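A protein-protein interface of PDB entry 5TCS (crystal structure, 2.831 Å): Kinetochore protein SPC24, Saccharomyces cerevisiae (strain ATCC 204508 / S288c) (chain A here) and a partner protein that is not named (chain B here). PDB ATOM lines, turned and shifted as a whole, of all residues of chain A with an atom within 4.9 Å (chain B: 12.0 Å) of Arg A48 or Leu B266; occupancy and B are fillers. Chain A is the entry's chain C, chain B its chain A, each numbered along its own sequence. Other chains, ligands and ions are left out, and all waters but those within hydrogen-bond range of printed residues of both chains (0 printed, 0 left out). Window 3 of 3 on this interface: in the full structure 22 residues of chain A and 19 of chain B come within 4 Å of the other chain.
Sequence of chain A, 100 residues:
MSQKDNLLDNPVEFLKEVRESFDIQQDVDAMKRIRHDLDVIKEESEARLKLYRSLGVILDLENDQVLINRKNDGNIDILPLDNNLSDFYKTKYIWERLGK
Glu A44 touches just one residue of chain B: Arg B267 (2.7 Å).
No residue of chain B comes within 4 Å of Ala A47.
Arg A48 touches one residue of chain B.
No residue of chain B comes within 4 Å of Leu A49.
No residue of chain B comes within 4 Å of Lys A50.
No residue of chain B comes within 4 Å of Leu A51.
No residue of chain B comes within 4 Å of Tyr A52.
Of the printed residues of chain A, Ile B263 touches Ile A41.
Of chain A, only Ile A41 (3.8 Å), Ser A45 (3.4 Å) and Arg A48 (3.2 Å) come within 4 Å of Leu B266.
Of the printed residues of chain A, Arg B267 touches Glu A44.
The nearest residue of chain B that does not touch Arg A48 is Leu B269 (4.8 Å).
O of Ile A41 is in hydrogen-bond range of OG of Ser A45 (2.8 Å).
O of Glu A44 is in hydrogen-bond range of NH2 of Arg A48 (2.7 Å).
Among the printed residues, merely in contact across the chains: Ser A45 with Leu B266, Ile A41 with Ile B263, Ile A41 with Val B262, Ile A41 with Leu B259 and Ile A41 with Leu B266.
Of the 15 printed residues of chain B, 5 touch a printed residue of chain A.
Along chain B the printed residues that touch a printed residue of chain A span positions 259 to 267.
Among the printed residues, 7 pairs touch across the chains.
Among the printed residues, Asp or Glu carboxylates within 4 Å of a Lys or Arg side-chain nitrogen of the other chain: Glu A44 with Arg B267.
The guanidinium group (NH2) of Arg A48 lies within hydrogen-bond range of the backbone carbonyl oxygen (O) of Leu B266 (3.2 Å).
NH2 of Arg B267 lies within salt-bridge range of OE2 of Glu A44, 2.7 Å away.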
ATOM      1  N   ILE A  41      12.354 -11.244 -16.109  1.00  0.00           N
ATOM      2  CA  ILE A  41      11.061 -10.765 -16.592  1.00  0.00           C
ATOM      3  C   ILE A  41       9.933 -11.612 -16.018  1.00  0.00           C
ATOM      4  O   ILE A  41       8.887 -11.089 -15.612  1.00  0.00           O
ATOM      5  CB  ILE A  41      11.045 -10.756 -18.132  1.00  0.00           C
ATOM      6  CG1 ILE A  41      12.110  -9.793 -18.660  1.00  0.00           C
ATOM      7  CG2 ILE A  41       9.668 -10.359 -18.656  1.00  0.00           C
ATOM      8  CD1 ILE A  41      12.365  -9.906 -20.143  1.00  0.00           C
ATOM      9  N   GLU A  44       9.630 -10.870 -12.055  1.00  0.00           N
ATOM     10  CA  GLU A  44       9.177  -9.509 -11.803  1.00  0.00           C
ATOM     11  C   GLU A  44       7.913  -9.144 -12.574  1.00  0.00           C
ATOM     12  O   GLU A  44       7.448  -8.005 -12.459  1.00  0.00           O
ATOM     13  CB  GLU A  44      10.299  -8.522 -12.138  1.00  0.00           C
ATOM     14  CG  GLU A  44      11.578  -8.774 -11.347  1.00  0.00           C
ATOM     15  CD  GLU A  44      12.619  -7.688 -11.536  1.00  0.00           C
ATOM     16  OE1 GLU A  44      12.277  -6.619 -12.085  1.00  0.00           O
ATOM     17  OE2 GLU A  44      13.781  -7.904 -11.131  1.00  0.00           O
ATOM     18  N   SER A  45       7.352 -10.071 -13.355  1.00  0.00           N
ATOM     19  CA  SER A  45       6.041  -9.886 -13.963  1.00  0.00           C
ATOM     20  C   SER A  45       4.954 -10.728 -13.310  1.00  0.00           C
ATOM     21  O   SER A  45       3.768 -10.427 -13.495  1.00  0.00           O
ATOM     22  CB  SER A  45       6.089 -10.230 -15.460  1.00  0.00           C
ATOM     23  OG  SER A  45       6.877  -9.299 -16.181  1.00  0.00           O
ATOM     24  N   GLU A  46       5.331 -11.757 -12.547  1.00  0.00           N
ATOM     25  CA  GLU A  46       4.364 -12.719 -12.023  1.00  0.00           C
ATOM     26  C   GLU A  46       3.175 -12.030 -11.360  1.00  0.00           C
ATOM     27  O   GLU A  46       2.023 -12.233 -11.759  1.00  0.00           O
ATOM     28  CB  GLU A  46       5.061 -13.655 -11.034  1.00  0.00           C
ATOM     29  CG  GLU A  46       4.203 -14.830 -10.590  1.00  0.00           C
ATOM     30  CD  GLU A  46       4.942 -15.770  -9.656  1.00  0.00           C
ATOM     31  OE1 GLU A  46       6.191 -15.743  -9.647  1.00  0.00           O
ATOM     32  OE2 GLU A  46       4.272 -16.533  -8.926  1.00  0.00           O
ATOM     33  N   ALA A  47       3.434 -11.212 -10.337  1.00  0.00           N
ATOM     34  CA  ALA A  47       2.345 -10.670  -9.528  1.00  0.00           C
ATOM     35  C   ALA A  47       1.431  -9.771 -10.353  1.00  0.00           C
ATOM     36  O   ALA A  47       0.206  -9.951 -10.362  1.00  0.00           O
ATOM     37  CB  ALA A  47       2.914  -9.906  -8.331  1.00  0.00           C
ATOM     38  N   ARG A  48       2.006  -8.788 -11.050  1.00  0.00           N
ATOM     39  CA  ARG A  48       1.190  -7.876 -11.846  1.00  0.00           C
ATOM     40  C   ARG A  48       0.358  -8.635 -12.871  1.00  0.00           C
ATOM     41  O   ARG A  48      -0.818  -8.313 -13.089  1.00  0.00           O
ATOM     42  CB  ARG A  48       2.081  -6.837 -12.529  1.00  0.00           C
ATOM     43  CG  ARG A  48       2.290  -5.574 -11.702  1.00  0.00           C
ATOM     44  CD  ARG A  48       3.395  -4.697 -12.266  1.00  0.00           C
ATOM     45  NE  ARG A  48       4.710  -5.315 -12.123  1.00  0.00           N
ATOM     46  CZ  ARG A  48       5.859  -4.707 -12.394  1.00  0.00           C
ATOM     47  NH1 ARG A  48       5.871  -3.452 -12.824  1.00  0.00           N
ATOM     48  NH2 ARG A  48       7.004  -5.354 -12.231  1.00  0.00           N
ATOM     49  N   LEU A  49       0.941  -9.655 -13.506  1.00  0.00           N
ATOM     50  CA  LEU A  49       0.171 -10.463 -14.445  1.00  0.00           C
ATOM     51  C   LEU A  49      -0.959 -11.199 -13.737  1.00  0.00           C
ATOM     52  O   LEU A  49      -2.060 -11.332 -14.283  1.00  0.00           O
ATOM     53  CB  LEU A  49       1.088 -11.453 -15.164  1.00  0.00           C
ATOM     54  CG  LEU A  49       2.057 -10.860 -16.191  1.00  0.00           C
ATOM     55  CD1 LEU A  49       2.971 -11.945 -16.734  1.00  0.00           C
ATOM     56  CD2 LEU A  49       1.305 -10.176 -17.330  1.00  0.00           C
ATOM     57  N   LYS A  50      -0.705 -11.689 -12.523  1.00  0.00           N
ATOM     58  CA  LYS A  50      -1.759 -12.343 -11.754  1.00  0.00           C
ATOM     59  C   LYS A  50      -2.900 -11.377 -11.474  1.00  0.00           C
ATOM     60  O   LYS A  50      -4.073 -11.770 -11.472  1.00  0.00           O
ATOM     61  CB  LYS A  50      -1.188 -12.891 -10.446  1.00  0.00           C
ATOM     62  CG  LYS A  50      -2.111 -13.850  -9.704  1.00  0.00           C
ATOM     63  CD  LYS A  50      -1.726 -14.001  -8.231  1.00  0.00           C
ATOM     64  CE  LYS A  50      -0.219 -14.170  -8.011  1.00  0.00           C
ATOM     65  NZ  LYS A  50       0.328 -15.418  -8.617  1.00  0.00           N
ATOM     66  N   LEU A  51      -2.577 -10.105 -11.236  1.00  0.00           N
ATOM     67  CA  LEU A  51      -3.615  -9.108 -10.993  1.00  0.00           C
ATOM     68  C   LEU A  51      -4.408  -8.823 -12.262  1.00  0.00           C
ATOM     69  O   LEU A  51      -5.644  -8.824 -12.247  1.00  0.00           O
ATOM     70  CB  LEU A  51      -2.989  -7.822 -10.448  1.00  0.00           C
ATOM     71  CG  LEU A  51      -3.935  -6.637 -10.237  1.00  0.00           C
ATOM     72  CD1 LEU A  51      -5.081  -7.011  -9.311  1.00  0.00           C
ATOM     73  CD2 LEU A  51      -3.176  -5.439  -9.685  1.00  0.00           C
ATOM     74  N   TYR A  52      -3.715  -8.578 -13.377  1.00  0.00           N
ATOM     75  CA  TYR A  52      -4.412  -8.262 -14.620  1.00  0.00           C
ATOM     76  C   TYR A  52      -5.281  -9.430 -15.078  1.00  0.00           C
ATOM     77  O   TYR A  52      -6.392  -9.224 -15.581  1.00  0.00           O
ATOM     78  CB  TYR A  52      -3.403  -7.877 -15.702  1.00  0.00           C
ATOM     79  CG  TYR A  52      -2.594  -6.640 -15.368  1.00  0.00           C
ATOM     80  CD1 TYR A  52      -3.163  -5.581 -14.671  1.00  0.00           C
ATOM     81  CD2 TYR A  52      -1.261  -6.537 -15.741  1.00  0.00           C
ATOM     82  CE1 TYR A  52      -2.429  -4.452 -14.362  1.00  0.00           C
ATOM     83  CE2 TYR A  52      -0.519  -5.410 -15.435  1.00  0.00           C
ATOM     84  CZ  TYR A  52      -1.108  -4.373 -14.745  1.00  0.00           C
ATOM     85  OH  TYR A  52      -0.373  -3.251 -14.438  1.00  0.00           O
ATOM     86  N   GLU B 256      19.397  -9.314 -26.265  1.00  0.00           N
ATOM     87  CA  GLU B 256      19.854  -8.768 -24.992  1.00  0.00           C
ATOM     88  C   GLU B 256      19.379  -7.337 -24.792  1.00  0.00           C
ATOM     89  O   GLU B 256      18.911  -6.977 -23.705  1.00  0.00           O
ATOM     90  CB  GLU B 256      21.377  -8.834 -24.913  1.00  0.00           C
ATOM     91  CG  GLU B 256      21.905 -10.177 -24.468  1.00  0.00           C
ATOM     92  CD  GLU B 256      23.280 -10.068 -23.858  1.00  0.00           C
ATOM     93  OE1 GLU B 256      24.266 -10.419 -24.538  1.00  0.00           O
ATOM     94  OE2 GLU B 256      23.376  -9.610 -22.701  1.00  0.00           O
ATOM     95  N   ASN B 257      19.485  -6.502 -25.828  1.00  0.00           N
ATOM     96  CA  ASN B 257      19.024  -5.124 -25.698  1.00  0.00           C
ATOM     97  C   ASN B 257      17.527  -5.088 -25.427  1.00  0.00           C
ATOM     98  O   ASN B 257      17.071  -4.493 -24.442  1.00  0.00           O
ATOM     99  CB  ASN B 257      19.373  -4.335 -26.962  1.00  0.00           C
ATOM    100  CG  ASN B 257      20.858  -4.052 -27.076  1.00  0.00           C
ATOM    101  OD1 ASN B 257      21.523  -3.769 -26.079  1.00  0.00           O
ATOM    102  ND2 ASN B 257      21.386  -4.129 -28.291  1.00  0.00           N
ATOM    103  N   GLU B 258      16.754  -5.766 -26.268  1.00  0.00           N
ATOM    104  CA  GLU B 258      15.307  -5.831 -26.130  1.00  0.00           C
ATOM    105  C   GLU B 258      14.889  -6.149 -24.704  1.00  0.00           C
ATOM    106  O   GLU B 258      14.302  -5.307 -24.012  1.00  0.00           O
ATOM    107  CB  GLU B 258      14.757  -6.889 -27.079  1.00  0.00           C
ATOM    108  CG  GLU B 258      14.722  -6.406 -28.483  1.00  0.00           C
ATOM    109  CD  GLU B 258      15.135  -7.448 -29.486  1.00  0.00           C
ATOM    110  OE1 GLU B 258      14.981  -8.649 -29.210  1.00  0.00           O
ATOM    111  OE2 GLU B 258      15.603  -7.050 -30.564  1.00  0.00           O
ATOM    112  N   LEU B 259      15.170  -7.381 -24.276  1.00  0.00           N
ATOM    113  CA  LEU B 259      14.849  -7.790 -22.916  1.00  0.00           C
ATOM    114  C   LEU B 259      15.310  -6.743 -21.913  1.00  0.00           C
ATOM    115  O   LEU B 259      14.570  -6.396 -20.984  1.00  0.00           O
ATOM    116  CB  LEU B 259      15.486  -9.151 -22.634  1.00  0.00           C
ATOM    117  CG  LEU B 259      15.099 -10.235 -23.652  1.00  0.00           C
ATOM    118  CD1 LEU B 259      15.812 -11.539 -23.368  1.00  0.00           C
ATOM    119  CD2 LEU B 259      13.591 -10.447 -23.675  1.00  0.00           C
ATOM    120  N   GLY B 260      16.512  -6.200 -22.109  1.00  0.00           N
ATOM    121  CA  GLY B 260      16.996  -5.121 -21.273  1.00  0.00           C
ATOM    122  C   GLY B 260      15.936  -4.057 -21.098  1.00  0.00           C
ATOM    123  O   GLY B 260      15.435  -3.847 -19.987  1.00  0.00           O
ATOM    124  N   ASN B 261      15.567  -3.404 -22.202  1.00  0.00           N
ATOM    125  CA  ASN B 261      14.498  -2.412 -22.162  1.00  0.00           C
ATOM    126  C   ASN B 261      13.318  -2.923 -21.346  1.00  0.00           C
ATOM    127  O   ASN B 261      12.876  -2.268 -20.397  1.00  0.00           O
ATOM    128  CB  ASN B 261      14.056  -2.059 -23.582  1.00  0.00           C
ATOM    129  CG  ASN B 261      15.195  -1.540 -24.439  1.00  0.00           C
ATOM    130  OD1 ASN B 261      16.125  -0.904 -23.940  1.00  0.00           O
ATOM    131  ND2 ASN B 261      15.127  -1.808 -25.739  1.00  0.00           N
ATOM    132  N   VAL B 262      12.814  -4.114 -21.688  1.00  0.00           N
ATOM    133  CA  VAL B 262      11.657  -4.668 -20.985  1.00  0.00           C
ATOM    134  C   VAL B 262      11.883  -4.596 -19.482  1.00  0.00           C
ATOM    135  O   VAL B 262      11.092  -4.005 -18.736  1.00  0.00           O
ATOM    136  CB  VAL B 262      11.385  -6.112 -21.445  1.00  0.00           C
ATOM    137  CG1 VAL B 262      10.357  -6.791 -20.541  1.00  0.00           C
ATOM    138  CG2 VAL B 262      10.901  -6.122 -22.883  1.00  0.00           C
ATOM    139  N   ILE B 263      12.994  -5.174 -19.022  1.00  0.00           N
ATOM    140  CA  ILE B 263      13.292  -5.184 -17.593  1.00  0.00           C
ATOM    141  C   ILE B 263      13.267  -3.763 -17.050  1.00  0.00           C
ATOM    142  O   ILE B 263      12.627  -3.474 -16.032  1.00  0.00           O
ATOM    143  CB  ILE B 263      14.642  -5.876 -17.335  1.00  0.00           C
ATOM    144  CG1 ILE B 263      14.488  -7.383 -17.550  1.00  0.00           C
ATOM    145  CG2 ILE B 263      15.148  -5.588 -15.919  1.00  0.00           C
ATOM    146  CD1 ILE B 263      15.792  -8.137 -17.635  1.00  0.00           C
ATOM    147  N   GLU B 264      13.947  -2.846 -17.742  1.00  0.00           N
ATOM    148  CA  GLU B 264      13.961  -1.456 -17.306  1.00  0.00           C
ATOM    149  C   GLU B 264      12.541  -0.947 -17.096  1.00  0.00           C
ATOM    150  O   GLU B 264      12.222  -0.357 -16.056  1.00  0.00           O
ATOM    151  CB  GLU B 264      14.700  -0.596 -18.333  1.00  0.00           C
ATOM    152  CG  GLU B 264      15.466   0.575 -17.733  1.00  0.00           C
ATOM    153  CD  GLU B 264      16.263   1.335 -18.773  1.00  0.00           C
ATOM    154  OE1 GLU B 264      15.737   2.331 -19.312  1.00  0.00           O
ATOM    155  OE2 GLU B 264      17.409   0.926 -19.061  1.00  0.00           O
ATOM    156  N   GLU B 265      11.661  -1.193 -18.070  1.00  0.00           N
ATOM    157  CA  GLU B 265      10.289  -0.714 -17.956  1.00  0.00           C
ATOM    158  C   GLU B 265       9.535  -1.437 -16.850  1.00  0.00           C
ATOM    159  O   GLU B 265       8.665  -0.840 -16.204  1.00  0.00           O
ATOM    160  CB  GLU B 265       9.573  -0.865 -19.296  1.00  0.00           C
ATOM    161  CG  GLU B 265       9.527   0.427 -20.097  1.00  0.00           C
ATOM    162  CD  GLU B 265       9.274   0.199 -21.575  1.00  0.00           C
ATOM    163  OE1 GLU B 265       9.139  -0.973 -21.985  1.00  0.00           O
ATOM    164  OE2 GLU B 265       9.211   1.194 -22.329  1.00  0.00           O
ATOM    165  N   LEU B 266       9.849  -2.711 -16.614  1.00  0.00           N
ATOM    166  CA  LEU B 266       9.261  -3.416 -15.483  1.00  0.00           C
ATOM    167  C   LEU B 266       9.717  -2.850 -14.147  1.00  0.00           C
ATOM    168  O   LEU B 266       9.103  -3.161 -13.121  1.00  0.00           O
ATOM    169  CB  LEU B 266       9.604  -4.906 -15.550  1.00  0.00           C
ATOM    170  CG  LEU B 266       8.759  -5.748 -16.505  1.00  0.00           C
ATOM    171  CD1 LEU B 266       9.410  -7.096 -16.748  1.00  0.00           C
ATOM    172  CD2 LEU B 266       7.358  -5.935 -15.950  1.00  0.00           C
ATOM    173  N   ARG B 267      10.767  -2.029 -14.135  1.00  0.00           N
ATOM    174  CA  ARG B 267      11.321  -1.488 -12.905  1.00  0.00           C
ATOM    175  C   ARG B 267      11.155   0.019 -12.791  1.00  0.00           C
ATOM    176  O   ARG B 267      11.557   0.598 -11.775  1.00  0.00           O
ATOM    177  CB  ARG B 267      12.806  -1.855 -12.801  1.00  0.00           C
ATOM    178  CG  ARG B 267      13.062  -3.354 -12.731  1.00  0.00           C
ATOM    179  CD  ARG B 267      14.546  -3.667 -12.638  1.00  0.00           C
ATOM    180  NE  ARG B 267      14.793  -5.085 -12.393  1.00  0.00           N
ATOM    181  CZ  ARG B 267      15.990  -5.659 -12.459  1.00  0.00           C
ATOM    182  NH1 ARG B 267      17.063  -4.944 -12.770  1.00  0.00           N
ATOM    183  NH2 ARG B 267      16.115  -6.956 -12.219  1.00  0.00           N
ATOM    184  N   ASN B 268      10.574   0.671 -13.795  1.00  0.00           N
ATOM    185  CA  ASN B 268      10.342   2.111 -13.748  1.00  0.00           C
ATOM    186  C   ASN B 268       9.084   2.375 -12.930  1.00  0.00           C
ATOM    187  O   ASN B 268       7.974   2.043 -13.361  1.00  0.00           O
ATOM    188  CB  ASN B 268      10.211   2.677 -15.157  1.00  0.00           C
ATOM    189  CG  ASN B 268      10.381   4.180 -15.199  1.00  0.00           C
ATOM    190  OD1 ASN B 268       9.889   4.896 -14.326  1.00  0.00           O
ATOM    191  ND2 ASN B 268      11.089   4.668 -16.211  1.00  0.00           N
ATOM    192  N   LEU B 269       9.253   2.971 -11.750  1.00  0.00           N
ATOM    193  CA  LEU B 269       8.162   3.158 -10.803  1.00  0.00           C
ATOM    194  C   LEU B 269       7.868   4.636 -10.565  1.00  0.00           C
ATOM    195  O   LEU B 269       7.513   5.036  -9.454  1.00  0.00           O
ATOM    196  CB  LEU B 269       8.485   2.458  -9.483  1.00  0.00           C
ATOM    197  CG  LEU B 269       9.004   1.023  -9.612  1.00  0.00           C
ATOM    198  CD1 LEU B 269       9.171   0.410  -8.243  1.00  0.00           C
ATOM    199  CD2 LEU B 269       8.085   0.160 -10.468  1.00  0.00           C
ATOM    200  N   GLU B 270       8.013   5.456 -11.602  1.00  0.00           N
ATOM    201  CA  GLU B 270       7.711   6.880 -11.510  1.00  0.00           C
ATOM    202  C   GLU B 270       6.308   7.118 -10.955  1.00  0.00           C
ATOM    203  O   GLU B 270       6.143   7.720  -9.892  1.00  0.00           O
ATOM    204  CB  GLU B 270       7.847   7.540 -12.884  1.00  0.00           C
ATOM    205  CG  GLU B 270       9.218   8.144 -13.146  1.00  0.00           C
ATOM    206  CD  GLU B 270       9.502   8.328 -14.625  1.00  0.00           C
ATOM    207  OE1 GLU B 270       8.539   8.344 -15.420  1.00  0.00           O
ATOM    208  OE2 GLU B 270      10.689   8.453 -14.992  1.00  0.00           O
